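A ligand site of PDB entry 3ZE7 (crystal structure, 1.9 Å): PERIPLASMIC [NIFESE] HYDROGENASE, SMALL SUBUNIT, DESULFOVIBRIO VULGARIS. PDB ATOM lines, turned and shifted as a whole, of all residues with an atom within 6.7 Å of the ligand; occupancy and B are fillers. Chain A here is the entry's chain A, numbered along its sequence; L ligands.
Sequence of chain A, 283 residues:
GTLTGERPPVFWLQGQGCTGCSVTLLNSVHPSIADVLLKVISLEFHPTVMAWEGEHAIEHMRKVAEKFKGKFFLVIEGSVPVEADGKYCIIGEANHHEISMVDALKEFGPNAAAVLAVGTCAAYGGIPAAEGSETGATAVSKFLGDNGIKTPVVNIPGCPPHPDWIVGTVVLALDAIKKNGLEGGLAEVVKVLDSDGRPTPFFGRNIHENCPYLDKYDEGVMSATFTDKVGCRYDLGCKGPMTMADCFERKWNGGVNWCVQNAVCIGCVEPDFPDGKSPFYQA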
ATOM      1  N   ILE A 207     -18.306   9.034  -5.952  1.00  0.00           N
ATOM      2  CA  ILE A 207     -17.947   8.324  -7.199  1.00  0.00           C
ATOM      3  C   ILE A 207     -18.894   7.152  -7.470  1.00  0.00           C
ATOM      4  O   ILE A 207     -19.495   7.055  -8.534  1.00  0.00           O
ATOM      5  CB  ILE A 207     -16.501   7.787  -7.191  1.00  0.00           C
ATOM      6  CG1 ILE A 207     -15.503   8.886  -7.515  1.00  0.00           C
ATOM      7  CG2 ILE A 207     -16.304   6.724  -8.253  1.00  0.00           C
ATOM      8  CD1 ILE A 207     -15.025   9.596  -6.340  1.00  0.00           C
ATOM      9  N   HIS A 208     -19.033   6.265  -6.483  1.00  0.00           N
ATOM     10  CA  HIS A 208     -19.833   5.053  -6.599  1.00  0.00           C
ATOM     11  C   HIS A 208     -21.304   5.294  -6.988  1.00  0.00           C
ATOM     12  O   HIS A 208     -21.866   4.561  -7.811  1.00  0.00           O
ATOM     13  CB  HIS A 208     -19.708   4.262  -5.294  1.00  0.00           C
ATOM     14  CG  HIS A 208     -20.557   3.036  -5.194  1.00  0.00           C
ATOM     15  ND1 HIS A 208     -20.255   1.853  -5.829  1.00  0.00           N
ATOM     16  CD2 HIS A 208     -21.686   2.788  -4.478  1.00  0.00           C
ATOM     17  CE1 HIS A 208     -21.156   0.940  -5.536  1.00  0.00           C
ATOM     18  NE2 HIS A 208     -22.047   1.485  -4.709  1.00  0.00           N
ATOM     19  N   GLU A 209     -21.924   6.322  -6.392  1.00  0.00           N
ATOM     20  CA  GLU A 209     -23.338   6.589  -6.674  1.00  0.00           C
ATOM     21  C   GLU A 209     -23.567   6.976  -8.128  1.00  0.00           C
ATOM     22  O   GLU A 209     -24.669   6.790  -8.661  1.00  0.00           O
ATOM     23  CB  GLU A 209     -23.914   7.677  -5.747  1.00  0.00           C
ATOM     24  CG  GLU A 209     -24.151   7.185  -4.323  1.00  0.00           C
ATOM     25  CD  GLU A 209     -24.466   8.303  -3.336  1.00  0.00           C
ATOM     26  OE1 GLU A 209     -24.524   9.482  -3.744  1.00  0.00           O
ATOM     27  OE2 GLU A 209     -24.642   7.995  -2.140  1.00  0.00           O
ATOM     28  N   CYS A 211     -21.352   5.893 -10.630  1.00  0.00           N
ATOM     29  CA  CYS A 211     -20.463   5.065 -11.438  1.00  0.00           C
ATOM     30  C   CYS A 211     -21.231   4.351 -12.547  1.00  0.00           C
ATOM     31  O   CYS A 211     -22.344   3.902 -12.348  1.00  0.00           O
ATOM     32  CB  CYS A 211     -19.723   4.061 -10.549  1.00  0.00           C
ATOM     33  SG  CYS A 211     -18.559   2.979 -11.419  1.00  0.00           S
ATOM     34  N   PRO A 212     -20.633   4.280 -13.750  1.00  0.00           N
ATOM     35  CA  PRO A 212     -21.277   3.572 -14.857  1.00  0.00           C
ATOM     36  C   PRO A 212     -21.360   2.055 -14.600  1.00  0.00           C
ATOM     37  O   PRO A 212     -22.069   1.355 -15.331  1.00  0.00           O
ATOM     38  CB  PRO A 212     -20.362   3.868 -16.058  1.00  0.00           C
ATOM     39  CG  PRO A 212     -19.030   4.273 -15.460  1.00  0.00           C
ATOM     40  CD  PRO A 212     -19.388   4.972 -14.160  1.00  0.00           C
ATOM     41  N   TYR A 213     -20.646   1.562 -13.590  1.00  0.00           N
ATOM     42  CA  TYR A 213     -20.648   0.136 -13.263  1.00  0.00           C
ATOM     43  C   TYR A 213     -21.564  -0.233 -12.080  1.00  0.00           C
ATOM     44  O   TYR A 213     -21.643  -1.406 -11.689  1.00  0.00           O
ATOM     45  CB  TYR A 213     -19.228  -0.369 -13.035  1.00  0.00           C
ATOM     46  CG  TYR A 213     -18.319  -0.049 -14.198  1.00  0.00           C
ATOM     47  CD1 TYR A 213     -18.446  -0.706 -15.413  1.00  0.00           C
ATOM     48  CD2 TYR A 213     -17.336   0.932 -14.087  1.00  0.00           C
ATOM     49  CE1 TYR A 213     -17.618  -0.403 -16.484  1.00  0.00           C
ATOM     50  CE2 TYR A 213     -16.508   1.243 -15.136  1.00  0.00           C
ATOM     51  CZ  TYR A 213     -16.652   0.572 -16.335  1.00  0.00           C
ATOM     52  OH  TYR A 213     -15.821   0.883 -17.395  1.00  0.00           O
ATOM     53  N   LEU A 214     -22.284   0.759 -11.563  1.00  0.00           N
ATOM     54  CA  LEU A 214     -23.210   0.549 -10.440  1.00  0.00           C
ATOM     55  C   LEU A 214     -24.244  -0.546 -10.696  1.00  0.00           C
ATOM     56  O   LEU A 214     -24.606  -1.288  -9.764  1.00  0.00           O
ATOM     57  CB  LEU A 214     -23.902   1.877 -10.061  1.00  0.00           C
ATOM     58  CG  LEU A 214     -24.803   1.846  -8.834  1.00  0.00           C
ATOM     59  CD1 LEU A 214     -24.035   1.350  -7.612  1.00  0.00           C
ATOM     60  CD2 LEU A 214     -25.398   3.220  -8.565  1.00  0.00           C
ATOM     61  N   ASP A 215     -24.747  -0.650 -11.929  1.00  0.00           N
ATOM     62  CA  ASP A 215     -25.672  -1.725 -12.270  1.00  0.00           C
ATOM     63  C   ASP A 215     -25.044  -3.095 -12.063  1.00  0.00           C
ATOM     64  O   ASP A 215     -25.687  -4.018 -11.544  1.00  0.00           O
ATOM     65  CB  ASP A 215     -26.281  -1.574 -13.686  1.00  0.00           C
ATOM     66  CG  ASP A 215     -25.233  -1.615 -14.799  1.00  0.00           C
ATOM     67  OD1 ASP A 215     -24.065  -1.234 -14.565  1.00  0.00           O
ATOM     68  OD2 ASP A 215     -25.596  -2.040 -15.921  1.00  0.00           O
ATOM     69  N   LYS A 216     -23.772  -3.238 -12.427  1.00  0.00           N
ATOM     70  CA  LYS A 216     -23.039  -4.484 -12.227  1.00  0.00           C
ATOM     71  C   LYS A 216     -22.837  -4.779 -10.741  1.00  0.00           C
ATOM     72  O   LYS A 216     -22.950  -5.946 -10.307  1.00  0.00           O
ATOM     73  CB  LYS A 216     -21.697  -4.464 -12.950  1.00  0.00           C
ATOM     74  CG  LYS A 216     -21.819  -4.341 -14.470  1.00  0.00           C
ATOM     75  CD  LYS A 216     -22.490  -5.578 -15.079  1.00  0.00           C
ATOM     76  CE  LYS A 216     -22.623  -5.434 -16.593  1.00  0.00           C
ATOM     77  NZ  LYS A 216     -23.497  -6.477 -17.191  1.00  0.00           N
ATOM     78  N   TYR A 217     -22.540  -3.741  -9.968  1.00  0.00           N
ATOM     79  CA  TYR A 217     -22.378  -3.857  -8.520  1.00  0.00           C
ATOM     80  C   TYR A 217     -23.673  -4.392  -7.912  1.00  0.00           C
ATOM     81  O   TYR A 217     -23.643  -5.351  -7.114  1.00  0.00           O
ATOM     82  CB  TYR A 217     -22.030  -2.491  -7.942  1.00  0.00           C
ATOM     83  CG  TYR A 217     -21.964  -2.392  -6.423  1.00  0.00           C
ATOM     84  CD1 TYR A 217     -23.094  -2.082  -5.674  1.00  0.00           C
ATOM     85  CD2 TYR A 217     -20.761  -2.578  -5.746  1.00  0.00           C
ATOM     86  CE1 TYR A 217     -23.032  -1.970  -4.281  1.00  0.00           C
ATOM     87  CE2 TYR A 217     -20.691  -2.459  -4.362  1.00  0.00           C
ATOM     88  CZ  TYR A 217     -21.835  -2.159  -3.637  1.00  0.00           C
ATOM     89  OH  TYR A 217     -21.759  -2.040  -2.272  1.00  0.00           O
ATOM     90  N   ASP A 218     -24.798  -3.795  -8.291  1.00  0.00           N
ATOM     91  CA  ASP A 218     -26.098  -4.207  -7.771  1.00  0.00           C
ATOM     92  C   ASP A 218     -26.486  -5.637  -8.172  1.00  0.00           C
ATOM     93  O   ASP A 218     -27.147  -6.348  -7.405  1.00  0.00           O
ATOM     94  CB  ASP A 218     -27.187  -3.215  -8.154  1.00  0.00           C
ATOM     95  CG  ASP A 218     -27.055  -1.889  -7.415  1.00  0.00           C
ATOM     96  OD1 ASP A 218     -26.378  -1.849  -6.360  1.00  0.00           O
ATOM     97  OD2 ASP A 218     -27.650  -0.895  -7.880  1.00  0.00           O
ATOM     98  N   MET A 222     -18.872  -9.154 -10.456  1.00  0.00           N
ATOM     99  CA  MET A 222     -17.553  -8.578 -10.187  1.00  0.00           C
ATOM    100  C   MET A 222     -16.466  -9.116 -11.117  1.00  0.00           C
ATOM    101  O   MET A 222     -16.326 -10.322 -11.277  1.00  0.00           O
ATOM    102  CB  MET A 222     -17.116  -8.917  -8.760  1.00  0.00           C
ATOM    103  CG  MET A 222     -18.164  -8.660  -7.717  1.00  0.00           C
ATOM    104  SD  MET A 222     -18.489  -6.895  -7.658  1.00  0.00           S
ATOM    105  CE  MET A 222     -20.271  -6.922  -7.625  1.00  0.00           C
ATOM    106  N   GLY A 231     -17.455  -6.147 -15.552  1.00  0.00           N
ATOM    107  CA  GLY A 231     -17.938  -6.183 -14.179  1.00  0.00           C
ATOM    108  C   GLY A 231     -17.559  -4.981 -13.317  1.00  0.00           C
ATOM    109  O   GLY A 231     -16.730  -4.152 -13.689  1.00  0.00           O
ATOM    110  N   CYS A 232     -18.198  -4.897 -12.156  1.00  0.00           N
ATOM    111  CA  CYS A 232     -17.808  -3.940 -11.118  1.00  0.00           C
ATOM    112  C   CYS A 232     -16.402  -4.280 -10.608  1.00  0.00           C
ATOM    113  O   CYS A 232     -16.001  -5.450 -10.605  1.00  0.00           O
ATOM    114  CB  CYS A 232     -18.834  -4.010  -9.985  1.00  0.00           C
ATOM    115  SG  CYS A 232     -18.389  -3.187  -8.439  1.00  0.00           S
ATOM    116  N   ARG A 233     -15.659  -3.260 -10.170  1.00  0.00           N
ATOM    117  CA  ARG A 233     -14.259  -3.428  -9.741  1.00  0.00           C
ATOM    118  C   ARG A 233     -14.114  -3.583  -8.213  1.00  0.00           C
ATOM    119  O   ARG A 233     -12.986  -3.558  -7.677  1.00  0.00           O
ATOM    120  CB  ARG A 233     -13.429  -2.217 -10.177  1.00  0.00           C
ATOM    121  CG  ARG A 233     -13.000  -2.185 -11.647  1.00  0.00           C
ATOM    122  CD  ARG A 233     -14.169  -1.949 -12.607  1.00  0.00           C
ATOM    123  NE  ARG A 233     -13.723  -1.309 -13.834  1.00  0.00           N
ATOM    124  CZ  ARG A 233     -14.256  -1.486 -15.032  1.00  0.00           C
ATOM    125  NH1 ARG A 233     -15.265  -2.337 -15.185  1.00  0.00           N
ATOM    126  NH2 ARG A 233     -13.763  -0.838 -16.080  1.00  0.00           N
ATOM    127  N   TYR A 234     -15.240  -3.740  -7.519  1.00  0.00           N
ATOM    128  CA  TYR A 234     -15.268  -3.839  -6.061  1.00  0.00           C
ATOM    129  C   TYR A 234     -14.370  -4.937  -5.468  1.00  0.00           C
ATOM    130  O   TYR A 234     -13.622  -4.676  -4.526  1.00  0.00           O
ATOM    131  CB  TYR A 234     -16.711  -4.024  -5.547  1.00  0.00           C
ATOM    132  CG  TYR A 234     -16.818  -4.121  -4.038  1.00  0.00           C
ATOM    133  CD1 TYR A 234     -16.846  -2.973  -3.254  1.00  0.00           C
ATOM    134  CD2 TYR A 234     -16.882  -5.349  -3.402  1.00  0.00           C
ATOM    135  CE1 TYR A 234     -16.939  -3.055  -1.887  1.00  0.00           C
ATOM    136  CE2 TYR A 234     -16.984  -5.439  -2.027  1.00  0.00           C
ATOM    137  CZ  TYR A 234     -17.012  -4.285  -1.274  1.00  0.00           C
ATOM    138  OH  TYR A 234     -17.115  -4.362   0.100  1.00  0.00           O
ATOM    139  N   ASP A 235     -14.454  -6.146  -6.000  1.00  0.00           N
ATOM    140  CA  ASP A 235     -13.593  -7.233  -5.522  1.00  0.00           C
ATOM    141  C   ASP A 235     -12.101  -6.992  -5.776  1.00  0.00           C
ATOM    142  O   ASP A 235     -11.246  -7.517  -5.058  1.00  0.00           O
ATOM    143  CB  ASP A 235     -14.012  -8.579  -6.120  1.00  0.00           C
ATOM    144  CG  ASP A 235     -15.251  -9.149  -5.485  1.00  0.00           C
ATOM    145  OD1 ASP A 235     -15.703  -8.598  -4.455  1.00  0.00           O
ATOM    146  OD2 ASP A 235     -15.774 -10.145  -6.009  1.00  0.00           O
ATOM    147  N   CYS A 238     -11.778  -1.599  -5.432  1.00  0.00           N
ATOM    148  CA  CYS A 238     -12.286  -0.257  -5.719  1.00  0.00           C
ATOM    149  C   CYS A 238     -12.856   0.465  -4.489  1.00  0.00           C
ATOM    150  O   CYS A 238     -13.716  -0.069  -3.772  1.00  0.00           O
ATOM    151  CB  CYS A 238     -13.303  -0.287  -6.857  1.00  0.00           C
ATOM    152  SG  CYS A 238     -13.886   1.346  -7.371  1.00  0.00           S
ATOM    153  N   LYS A 239     -12.365   1.676  -4.240  1.00  0.00           N
ATOM    154  CA  LYS A 239     -12.774   2.494  -3.103  1.00  0.00           C
ATOM    155  C   LYS A 239     -13.787   3.580  -3.478  1.00  0.00           C
ATOM    156  O   LYS A 239     -14.043   4.493  -2.676  1.00  0.00           O
ATOM    157  CB  LYS A 239     -11.553   3.155  -2.449  1.00  0.00           C
ATOM    158  CG  LYS A 239     -10.533   2.171  -1.951  1.00  0.00           C
ATOM    159  CD  LYS A 239     -11.198   1.026  -1.172  1.00  0.00           C
ATOM    160  CE  LYS A 239     -10.131   0.142  -0.508  1.00  0.00           C
ATOM    161  NZ  LYS A 239      -9.084  -0.360  -1.471  1.00  0.00           N
ATOM    162  N   GLY A 240     -14.337   3.494  -4.683  1.00  0.00           N
ATOM    163  CA  GLY A 240     -15.418   4.371  -5.101  1.00  0.00           C
ATOM    164  C   GLY A 240     -16.492   4.605  -4.033  1.00  0.00           C
ATOM    165  O   GLY A 240     -16.860   5.752  -3.767  1.00  0.00           O
ATOM    166  N   PRO A 241     -17.000   3.509  -3.419  1.00  0.00           N
ATOM    167  CA  PRO A 241     -18.056   3.678  -2.417  1.00  0.00           C
ATOM    168  C   PRO A 241     -17.728   4.669  -1.302  1.00  0.00           C
ATOM    169  O   PRO A 241     -18.650   5.250  -0.755  1.00  0.00           O
ATOM    170  CB  PRO A 241     -18.233   2.270  -1.858  1.00  0.00           C
ATOM    171  CG  PRO A 241     -17.899   1.394  -2.993  1.00  0.00           C
ATOM    172  CD  PRO A 241     -16.747   2.080  -3.686  1.00  0.00           C
ATOM    173  N   TRP A 258      -9.957   7.157 -16.885  1.00  0.00           N
ATOM    174  CA  TRP A 258     -10.067   7.475 -15.464  1.00  0.00           C
ATOM    175  C   TRP A 258      -9.854   6.198 -14.688  1.00  0.00           C
ATOM    176  O   TRP A 258      -9.881   5.106 -15.261  1.00  0.00           O
ATOM    177  CB  TRP A 258     -11.392   8.183 -15.092  1.00  0.00           C
ATOM    178  CG  TRP A 258     -12.649   7.344 -15.096  1.00  0.00           C
ATOM    179  CD1 TRP A 258     -13.202   6.689 -16.179  1.00  0.00           C
ATOM    180  CD2 TRP A 258     -13.558   7.113 -13.998  1.00  0.00           C
ATOM    181  NE1 TRP A 258     -14.372   6.060 -15.803  1.00  0.00           N
ATOM    182  CE2 TRP A 258     -14.615   6.308 -14.488  1.00  0.00           C
ATOM    183  CE3 TRP A 258     -13.574   7.499 -12.657  1.00  0.00           C
ATOM    184  CZ2 TRP A 258     -15.661   5.875 -13.670  1.00  0.00           C
ATOM    185  CZ3 TRP A 258     -14.627   7.086 -11.852  1.00  0.00           C
ATOM    186  CH2 TRP A 258     -15.656   6.276 -12.355  1.00  0.00           C
ATOM    187  N   VAL A 260     -11.262   4.253 -12.498  1.00  0.00           N
ATOM    188  CA  VAL A 260     -12.188   3.121 -12.371  1.00  0.00           C
ATOM    189  C   VAL A 260     -12.279   2.327 -13.686  1.00  0.00           C
ATOM    190  O   VAL A 260     -12.313   1.099 -13.685  1.00  0.00           O
ATOM    191  CB  VAL A 260     -13.580   3.566 -11.884  1.00  0.00           C
ATOM    192  CG1 VAL A 260     -14.596   2.418 -11.988  1.00  0.00           C
ATOM    193  CG2 VAL A 260     -13.502   4.089 -10.428  1.00  0.00           C
ATOM    194  N   ALA A 263      -8.518   0.689 -13.943  1.00  0.00           N
ATOM    195  CA  ALA A 263      -8.096  -0.192 -12.854  1.00  0.00           C
ATOM    196  C   ALA A 263      -9.095  -0.080 -11.710  1.00  0.00           C
ATOM    197  O   ALA A 263     -10.210  -0.590 -11.810  1.00  0.00           O
ATOM    198  CB  ALA A 263      -6.675   0.143 -12.394  1.00  0.00           C
ATOM    199  N   CYS A 265     -10.488   2.790  -8.328  1.00  0.00           N
ATOM    200  CA  CYS A 265     -10.336   4.014  -7.539  1.00  0.00           C
ATOM    201  C   CYS A 265      -9.610   3.662  -6.219  1.00  0.00           C
ATOM    202  O   CYS A 265      -9.915   2.651  -5.605  1.00  0.00           O
ATOM    203  CB  CYS A 265     -11.704   4.656  -7.250  1.00  0.00           C
ATOM    204  SG  CYS A 265     -11.676   6.123  -6.129  1.00  0.00           S
HETATM  205 FE1  LIG L   1     -16.148   0.942  -7.934  1.00  0.00          FE
HETATM  206 FE2  LIG L   1     -18.077  -0.930  -8.605  1.00  0.00          FE
HETATM  207 FE3  LIG L   1     -18.083   1.586  -9.707  1.00  0.00          FE
HETATM  208 FE4  LIG L   1     -18.719   1.246  -7.111  1.00  0.00          FE
HETATM  209  S1  LIG L   1     -19.895   0.398  -8.918  1.00  0.00           S
HETATM  210  S2  LIG L   1     -17.361   2.898  -7.947  1.00  0.00           S
HETATM  211  S3  LIG L   1     -17.292  -0.437  -6.479  1.00  0.00           S
HETATM  212  S4  LIG L   1     -16.480  -0.029 -10.004  1.00  0.00           S
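The backbone carbonyl oxygen (O) of Tyr 213 sits close to a sulfur (S1) of the ligand (3.7 Å).
Residues that only touch the ligand: Val 260, Tyr 217, Gly 240, Tyr 234, Pro 241 and Ile 207.
The nearest printed residue that does not touch the ligand is Lys 239 (5.3 Å).
The backbone NH of Arg 233 lies close to a sulfur (S4) of the ligand, 3.3 Å away.
The side-chain sulfur (SG) of Cys 238 is bound to an iron atom (FE1) of the ligand, 2.4 Å away.
FE4 of the ligand is bound by ND1 of His 208 (2.1 Å).
FE2 of the ligand is bound by SG of Cys 232, 2.3 Å away.
The backbone NH (N) of Leu 214 sits close to a sulfur (S1) of the ligand (3.6 Å).
SG of Cys 211 is bound to FE3 of the ligand.
The backbone NH (N) of Tyr 213 sits close to the side-chain sulfur (SG) of Cys 211 (3.3 Å).
The side-chain sulfur of Cys 232 lies close to the side-chain sulfur of Met 222 (3.8 Å).
OH of Tyr 213 lies within hydrogen-bond range of NH2 of Arg 233 (3.0 Å).
N of Gly 240 lies close to SG of Cys 238, at 3.5 Å.
The guanidinium group of Arg 233 lies within hydrogen-bond range of the backbone carbonyl oxygen of Gly 231, at 2.8 Å.
The guanidinium group (NE) of Arg 233 sits at hydrogen-bond distance from the backbone carbonyl oxygen (O) of Val 260 (2.8 Å).
The backbone NH of Tyr 234 lies close to the side-chain sulfur of Cys 232, at 3.3 Å.
The backbone carbonyl oxygen of Arg 233 sits at hydrogen-bond distance from the backbone NH of Cys 238, 3.2 Å away.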
